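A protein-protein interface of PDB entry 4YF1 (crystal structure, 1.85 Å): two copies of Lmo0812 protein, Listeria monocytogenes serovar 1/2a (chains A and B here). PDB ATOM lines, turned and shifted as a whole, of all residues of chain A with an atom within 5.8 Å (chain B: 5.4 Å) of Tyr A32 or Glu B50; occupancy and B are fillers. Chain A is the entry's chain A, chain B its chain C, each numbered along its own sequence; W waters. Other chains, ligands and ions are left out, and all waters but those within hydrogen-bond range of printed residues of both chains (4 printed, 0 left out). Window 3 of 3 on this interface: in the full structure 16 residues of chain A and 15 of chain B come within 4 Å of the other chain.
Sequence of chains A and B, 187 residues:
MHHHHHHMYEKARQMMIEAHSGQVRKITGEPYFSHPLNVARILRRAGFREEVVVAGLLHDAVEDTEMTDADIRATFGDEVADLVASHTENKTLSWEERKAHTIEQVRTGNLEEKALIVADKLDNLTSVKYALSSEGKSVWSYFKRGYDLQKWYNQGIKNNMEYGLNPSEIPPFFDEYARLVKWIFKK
Glu B50 touches Tyr A32 (CG to OH, 3.3 Å). Tyr A32 touches Glu B51. Leu A37 touches Val B54 (CD1 to CG2, 3.5 Å).
Arg B44 touches its own counterpart, Arg A44. Position printed for both chains: 44. Of the 5 pairs that touch across the chains among the printed residues, 1 has its exchanged pair printed and touching as well.
The side-chain amide oxygen of Asn A38 sits at hydrogen-bond distance from the backbone NH of Tyr A32 (3.0 Å). The guanidinium group (NE) of Arg B44 is in salt-bridge range of the side-chain carboxylate (OE2) of Glu B50 (2.7 Å). The guanidinium group (NH1) of Arg B49 is in salt-bridge range of the side-chain carboxylate (OE1) of Glu B51, at 3.5 Å.
The guanidinium group (NH2) of Arg A44 is in salt-bridge range of the side-chain carboxylate (OE1) of Glu B50 (3.7 Å). The guanidinium group (NH2) of Arg A44 lies close to the guanidinium group (NH2) of Arg B44, 3.3 Å away.
Water W2 lies within hydrogen-bond range of the side-chain carboxylate of Glu B51 (2.7 Å) and the backbone carbonyl oxygen of Tyr A32 (2.9 Å). Water W1 lies within hydrogen-bond range of OH of Tyr A32 (2.8 Å) and N of Glu B50 (2.9 Å). Water W4 lies within hydrogen-bond range of NH2 of Arg A44 (3.0 Å) and OE1 of Glu B50 (3.1 Å). Water W3 lies within hydrogen-bond range of NH2 of Arg A44 (3.1 Å) and NH2 of Arg B44 (3.2 Å).
Tyr A32 touches two residues of chain B. Printed residues of chain B within 4 Å of Arg A44: Arg B44 and Glu B50. Of the printed residues of chain A, Arg B44 touches Arg A44 (3.3 Å). Printed residues of chain A within 4 Å of Glu B50: Tyr A32 and Arg A44. Printed residues of chain A within 4 Å of Glu B51: Tyr A32 (3.5 Å). Printed residues of chain A within 4 Å of Val B54: Leu A37 (3.5 Å). Ala B55 touches none of the printed residues of chain A. The nearest printed residue of chain A that does not touch Glu B50 is Leu A37 (4.5 Å).
Of the 10 printed residues of chain A, 3 touch a printed residue of chain B. Printed residues of chain A that touch a printed residue of chain B: Tyr A32, Leu A37 and Arg A44. Hydrophobic or aromatic side chains of chain A within 4 Å of the printed part of chain B: Tyr A32 and Leu A37. Along chain A the printed residues that touch a printed residue of chain B span positions 32 to 44. Of the 9 printed residues of chain B, 4 touch a printed residue of chain A. Among the printed residues, Asp or Glu carboxylates within 4 Å of a Lys or Arg side-chain nitrogen of the other chain: Arg A44 with Glu B50 (3.7 Å).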
ATOM      1  N   GLY A  29     -18.641  -1.272 -14.150  1.00  0.00           N
ATOM      2  CA  GLY A  29     -19.270  -2.532 -13.766  1.00  0.00           C
ATOM      3  C   GLY A  29     -19.484  -3.614 -14.818  1.00  0.00           C
ATOM      4  O   GLY A  29     -18.770  -3.716 -15.810  1.00  0.00           O
ATOM      5  N   GLU A  30     -20.524  -4.391 -14.576  1.00  0.00           N
ATOM      6  CA  GLU A  30     -20.828  -5.553 -15.367  1.00  0.00           C
ATOM      7  C   GLU A  30     -21.293  -5.191 -16.780  1.00  0.00           C
ATOM      8  O   GLU A  30     -21.870  -4.131 -16.996  1.00  0.00           O
ATOM      9  CB  GLU A  30     -21.834  -6.446 -14.604  1.00  0.00           C
ATOM     10  CG  GLU A  30     -23.241  -5.914 -14.459  1.00  0.00           C
ATOM     11  CD  GLU A  30     -24.068  -6.712 -13.433  1.00  0.00           C
ATOM     12  OE1 GLU A  30     -23.558  -6.975 -12.306  1.00  0.00           O
ATOM     13  OE2 GLU A  30     -25.250  -7.047 -13.728  1.00  0.00           O
ATOM     14  N   PRO A  31     -21.122  -6.091 -17.739  1.00  0.00           N
ATOM     15  CA  PRO A  31     -20.585  -7.441 -17.569  1.00  0.00           C
ATOM     16  C   PRO A  31     -19.076  -7.597 -17.762  1.00  0.00           C
ATOM     17  O   PRO A  31     -18.550  -8.622 -17.387  1.00  0.00           O
ATOM     18  CB  PRO A  31     -21.297  -8.228 -18.717  1.00  0.00           C
ATOM     19  CG  PRO A  31     -21.422  -7.202 -19.800  1.00  0.00           C
ATOM     20  CD  PRO A  31     -21.766  -5.908 -19.058  1.00  0.00           C
ATOM     21  N   TYR A  32     -18.396  -6.633 -18.372  1.00  0.00           N
ATOM     22  CA  TYR A  32     -16.956  -6.778 -18.638  1.00  0.00           C
ATOM     23  C   TYR A  32     -15.980  -6.067 -17.701  1.00  0.00           C
ATOM     24  O   TYR A  32     -14.778  -6.298 -17.808  1.00  0.00           O
ATOM     25  CB  TYR A  32     -16.641  -6.421 -20.078  1.00  0.00           C
ATOM     26  CG  TYR A  32     -17.251  -7.409 -21.059  1.00  0.00           C
ATOM     27  CD1 TYR A  32     -16.820  -8.728 -21.094  1.00  0.00           C
ATOM     28  CD2 TYR A  32     -18.239  -7.018 -21.966  1.00  0.00           C
ATOM     29  CE1 TYR A  32     -17.367  -9.644 -21.991  1.00  0.00           C
ATOM     30  CE2 TYR A  32     -18.783  -7.932 -22.873  1.00  0.00           C
ATOM     31  CZ  TYR A  32     -18.349  -9.249 -22.856  1.00  0.00           C
ATOM     32  OH  TYR A  32     -18.872 -10.168 -23.752  1.00  0.00           O
ATOM     33  N   PHE A  33     -16.483  -5.214 -16.817  1.00  0.00           N
ATOM     34  CA  PHE A  33     -15.632  -4.503 -15.843  1.00  0.00           C
ATOM     35  C   PHE A  33     -14.512  -3.726 -16.508  1.00  0.00           C
ATOM     36  O   PHE A  33     -13.383  -3.689 -16.047  1.00  0.00           O
ATOM     37  CB  PHE A  33     -15.119  -5.481 -14.791  1.00  0.00           C
ATOM     38  CG  PHE A  33     -16.226  -6.193 -14.102  1.00  0.00           C
ATOM     39  CD1 PHE A  33     -16.905  -5.582 -13.065  1.00  0.00           C
ATOM     40  CD2 PHE A  33     -16.665  -7.427 -14.558  1.00  0.00           C
ATOM     41  CE1 PHE A  33     -17.973  -6.217 -12.453  1.00  0.00           C
ATOM     42  CE2 PHE A  33     -17.741  -8.058 -13.960  1.00  0.00           C
ATOM     43  CZ  PHE A  33     -18.394  -7.457 -12.906  1.00  0.00           C
ATOM     44  N   SER A  34     -14.886  -3.108 -17.617  1.00  0.00           N
ATOM     45  CA  SER A  34     -14.004  -2.337 -18.452  1.00  0.00           C
ATOM     46  C   SER A  34     -14.901  -1.468 -19.320  1.00  0.00           C
ATOM     47  O   SER A  34     -15.790  -1.983 -19.981  1.00  0.00           O
ATOM     48  CB  SER A  34     -13.193  -3.288 -19.326  1.00  0.00           C
ATOM     49  OG  SER A  34     -12.524  -2.606 -20.352  1.00  0.00           O
ATOM     50  N   LEU A  37     -14.865  -2.414 -23.234  1.00  0.00           N
ATOM     51  CA  LEU A  37     -15.568  -3.652 -23.512  1.00  0.00           C
ATOM     52  C   LEU A  37     -17.079  -3.478 -23.367  1.00  0.00           C
ATOM     53  O   LEU A  37     -17.840  -4.000 -24.157  1.00  0.00           O
ATOM     54  CB  LEU A  37     -15.034  -4.784 -22.629  1.00  0.00           C
ATOM     55  CG  LEU A  37     -13.677  -5.370 -23.053  1.00  0.00           C
ATOM     56  CD1 LEU A  37     -13.854  -6.167 -24.320  1.00  0.00           C
ATOM     57  CD2 LEU A  37     -12.594  -4.340 -23.269  1.00  0.00           C
ATOM     58  N   ASN A  38     -17.503  -2.743 -22.333  1.00  0.00           N
ATOM     59  CA  ASN A  38     -18.942  -2.498 -22.139  1.00  0.00           C
ATOM     60  C   ASN A  38     -19.555  -1.612 -23.216  1.00  0.00           C
ATOM     61  O   ASN A  38     -20.697  -1.826 -23.622  1.00  0.00           O
ATOM     62  CB  ASN A  38     -19.244  -1.863 -20.743  1.00  0.00           C
ATOM     63  CG  ASN A  38     -19.107  -2.840 -19.579  1.00  0.00           C
ATOM     64  OD1 ASN A  38     -18.969  -4.047 -19.745  1.00  0.00           O
ATOM     65  ND2 ASN A  38     -19.197  -2.292 -18.337  1.00  0.00           N
ATOM     66  N   ARG A  41     -19.942  -3.743 -26.348  1.00  0.00           N
ATOM     67  CA  ARG A  41     -21.127  -4.571 -26.209  1.00  0.00           C
ATOM     68  C   ARG A  41     -22.425  -3.834 -26.531  1.00  0.00           C
ATOM     69  O   ARG A  41     -23.306  -4.373 -27.225  1.00  0.00           O
ATOM     70  CB  ARG A  41     -21.184  -5.202 -24.802  1.00  0.00           C
ATOM     71  CG  ARG A  41     -22.456  -5.940 -24.471  1.00  0.00           C
ATOM     72  CD  ARG A  41     -22.435  -6.618 -23.104  1.00  0.00           C
ATOM     73  NE  ARG A  41     -23.756  -7.137 -22.801  1.00  0.00           N
ATOM     74  CZ  ARG A  41     -24.782  -6.392 -22.406  1.00  0.00           C
ATOM     75  NH1 ARG A  41     -24.620  -5.074 -22.140  1.00  0.00           N
ATOM     76  NH2 ARG A  41     -25.958  -6.969 -22.191  1.00  0.00           N
ATOM     77  N   ARG A  44     -22.512  -3.419 -30.314  1.00  0.00           N
ATOM     78  CA  ARG A  44     -22.685  -4.712 -31.018  1.00  0.00           C
ATOM     79  C   ARG A  44     -24.122  -5.141 -30.898  1.00  0.00           C
ATOM     80  O   ARG A  44     -24.770  -5.509 -31.892  1.00  0.00           O
ATOM     81  CB  ARG A  44     -21.716  -5.776 -30.451  1.00  0.00           C
ATOM     82  CG  ARG A  44     -21.936  -7.193 -30.979  1.00  0.00           C
ATOM     83  CD  ARG A  44     -20.898  -8.200 -30.505  1.00  0.00           C
ATOM     84  NE  ARG A  44     -20.571  -8.066 -29.074  1.00  0.00           N
ATOM     85  CZ  ARG A  44     -19.490  -7.474 -28.584  1.00  0.00           C
ATOM     86  NH1 ARG A  44     -19.299  -7.420 -27.254  1.00  0.00           N
ATOM     87  NH2 ARG A  44     -18.608  -6.882 -29.389  1.00  0.00           N
ATOM     88  N   ARG B  44     -14.458 -14.459 -32.892  1.00  0.00           N
ATOM     89  CA  ARG B  44     -15.857 -14.355 -32.480  1.00  0.00           C
ATOM     90  C   ARG B  44     -16.731 -15.461 -33.107  1.00  0.00           C
ATOM     91  O   ARG B  44     -17.555 -16.080 -32.415  1.00  0.00           O
ATOM     92  CB  ARG B  44     -16.434 -12.962 -32.772  1.00  0.00           C
ATOM     93  CG  ARG B  44     -17.878 -12.839 -32.303  1.00  0.00           C
ATOM     94  CD  ARG B  44     -18.458 -11.434 -32.393  1.00  0.00           C
ATOM     95  NE  ARG B  44     -17.747 -10.406 -31.596  1.00  0.00           N
ATOM     96  CZ  ARG B  44     -16.969  -9.438 -32.094  1.00  0.00           C
ATOM     97  NH1 ARG B  44     -16.753  -9.322 -33.407  1.00  0.00           N
ATOM     98  NH2 ARG B  44     -16.404  -8.554 -31.276  1.00  0.00           N
ATOM     99  N   PHE B  48     -15.255 -17.805 -29.145  1.00  0.00           N
ATOM    100  CA  PHE B  48     -14.433 -17.355 -28.031  1.00  0.00           C
ATOM    101  C   PHE B  48     -15.030 -16.154 -27.338  1.00  0.00           C
ATOM    102  O   PHE B  48     -15.719 -15.347 -27.958  1.00  0.00           O
ATOM    103  CB  PHE B  48     -12.991 -17.082 -28.452  1.00  0.00           C
ATOM    104  CG  PHE B  48     -12.248 -18.325 -28.747  1.00  0.00           C
ATOM    105  CD1 PHE B  48     -11.687 -19.061 -27.722  1.00  0.00           C
ATOM    106  CD2 PHE B  48     -12.210 -18.826 -30.030  1.00  0.00           C
ATOM    107  CE1 PHE B  48     -11.063 -20.256 -27.969  1.00  0.00           C
ATOM    108  CE2 PHE B  48     -11.580 -20.021 -30.293  1.00  0.00           C
ATOM    109  CZ  PHE B  48     -11.010 -20.741 -29.260  1.00  0.00           C
ATOM    110  N   ARG B  49     -14.745 -16.049 -26.039  1.00  0.00           N
ATOM    111  CA  ARG B  49     -15.285 -14.947 -25.261  1.00  0.00           C
ATOM    112  C   ARG B  49     -14.687 -13.618 -25.735  1.00  0.00           C
ATOM    113  O   ARG B  49     -13.586 -13.585 -26.301  1.00  0.00           O
ATOM    114  CB  ARG B  49     -15.030 -15.172 -23.774  1.00  0.00           C
ATOM    115  CG  ARG B  49     -13.565 -15.169 -23.402  1.00  0.00           C
ATOM    116  CD  ARG B  49     -13.393 -15.615 -21.971  1.00  0.00           C
ATOM    117  NE  ARG B  49     -11.986 -15.835 -21.638  1.00  0.00           N
ATOM    118  CZ  ARG B  49     -11.253 -15.116 -20.798  1.00  0.00           C
ATOM    119  NH1 ARG B  49     -11.769 -14.104 -20.103  1.00  0.00           N
ATOM    120  NH2 ARG B  49      -9.983 -15.458 -20.599  1.00  0.00           N
ATOM    121  N   GLU B  50     -15.370 -12.507 -25.440  1.00  0.00           N
ATOM    122  CA  GLU B  50     -14.925 -11.201 -25.975  1.00  0.00           C
ATOM    123  C   GLU B  50     -13.543 -10.741 -25.570  1.00  0.00           C
ATOM    124  O   GLU B  50     -12.902 -10.060 -26.341  1.00  0.00           O
ATOM    125  CB  GLU B  50     -15.977 -10.110 -25.769  1.00  0.00           C
ATOM    126  CG  GLU B  50     -17.234 -10.341 -26.620  1.00  0.00           C
ATOM    127  CD  GLU B  50     -16.995 -10.177 -28.131  1.00  0.00           C
ATOM    128  OE1 GLU B  50     -16.051  -9.475 -28.547  1.00  0.00           O
ATOM    129  OE2 GLU B  50     -17.789 -10.758 -28.907  1.00  0.00           O
ATOM    130  N   GLU B  51     -13.071 -11.115 -24.386  1.00  0.00           N
ATOM    131  CA  GLU B  51     -11.718 -10.760 -24.010  1.00  0.00           C
ATOM    132  C   GLU B  51     -10.685 -11.373 -24.972  1.00  0.00           C
ATOM    133  O   GLU B  51      -9.655 -10.758 -25.259  1.00  0.00           O
ATOM    134  CB  GLU B  51     -11.405 -11.160 -22.584  1.00  0.00           C
ATOM    135  CG  GLU B  51     -12.246 -10.404 -21.549  1.00  0.00           C
ATOM    136  CD  GLU B  51     -13.541 -11.090 -21.132  1.00  0.00           C
ATOM    137  OE1 GLU B  51     -14.037 -12.022 -21.814  1.00  0.00           O
ATOM    138  OE2 GLU B  51     -14.061 -10.670 -20.068  1.00  0.00           O
ATOM    139  N   VAL B  52     -10.969 -12.582 -25.463  1.00  0.00           N
ATOM    140  CA  VAL B  52     -10.069 -13.259 -26.403  1.00  0.00           C
ATOM    141  C   VAL B  52     -10.169 -12.537 -27.751  1.00  0.00           C
ATOM    142  O   VAL B  52      -9.172 -12.295 -28.406  1.00  0.00           O
ATOM    143  CB  VAL B  52     -10.425 -14.767 -26.567  1.00  0.00           C
ATOM    144  CG1 VAL B  52      -9.599 -15.411 -27.685  1.00  0.00           C
ATOM    145  CG2 VAL B  52     -10.220 -15.516 -25.260  1.00  0.00           C
ATOM    146  N   VAL B  53     -11.389 -12.216 -28.155  1.00  0.00           N
ATOM    147  CA  VAL B  53     -11.628 -11.500 -29.396  1.00  0.00           C
ATOM    148  C   VAL B  53     -10.876 -10.173 -29.379  1.00  0.00           C
ATOM    149  O   VAL B  53     -10.203  -9.819 -30.335  1.00  0.00           O
ATOM    150  CB  VAL B  53     -13.143 -11.253 -29.611  1.00  0.00           C
ATOM    151  CG1 VAL B  53     -13.390 -10.393 -30.841  1.00  0.00           C
ATOM    152  CG2 VAL B  53     -13.891 -12.568 -29.740  1.00  0.00           C
ATOM    153  N   VAL B  54     -10.973  -9.448 -28.261  1.00  0.00           N
ATOM    154  CA  VAL B  54     -10.308  -8.162 -28.146  1.00  0.00           C
ATOM    155  C   VAL B  54      -8.791  -8.302 -28.089  1.00  0.00           C
ATOM    156  O   VAL B  54      -8.073  -7.494 -28.685  1.00  0.00           O
ATOM    157  CB  VAL B  54     -10.889  -7.365 -26.968  1.00  0.00           C
ATOM    158  CG1 VAL B  54     -10.034  -6.151 -26.637  1.00  0.00           C
ATOM    159  CG2 VAL B  54     -12.319  -6.985 -27.312  1.00  0.00           C
ATOM    160  N   ALA B  55      -8.291  -9.305 -27.381  1.00  0.00           N
ATOM    161  CA  ALA B  55      -6.862  -9.545 -27.343  1.00  0.00           C
ATOM    162  C   ALA B  55      -6.325  -9.798 -28.787  1.00  0.00           C
ATOM    163  O   ALA B  55      -5.221  -9.365 -29.148  1.00  0.00           O
ATOM    164  CB  ALA B  55      -6.560 -10.731 -26.460  1.00  0.00           C
HETATM  165  O   HOH W   1     -17.731 -12.726 -23.733  1.00  0.00           O
HETATM  166  O   HOH W   2     -13.159  -8.391 -18.885  1.00  0.00           O
HETATM  167  O   HOH W   3     -18.719  -6.648 -32.516  1.00  0.00           O
HETATM  168  O   HOH W   4     -15.956  -6.362 -28.187  1.00  0.00           O
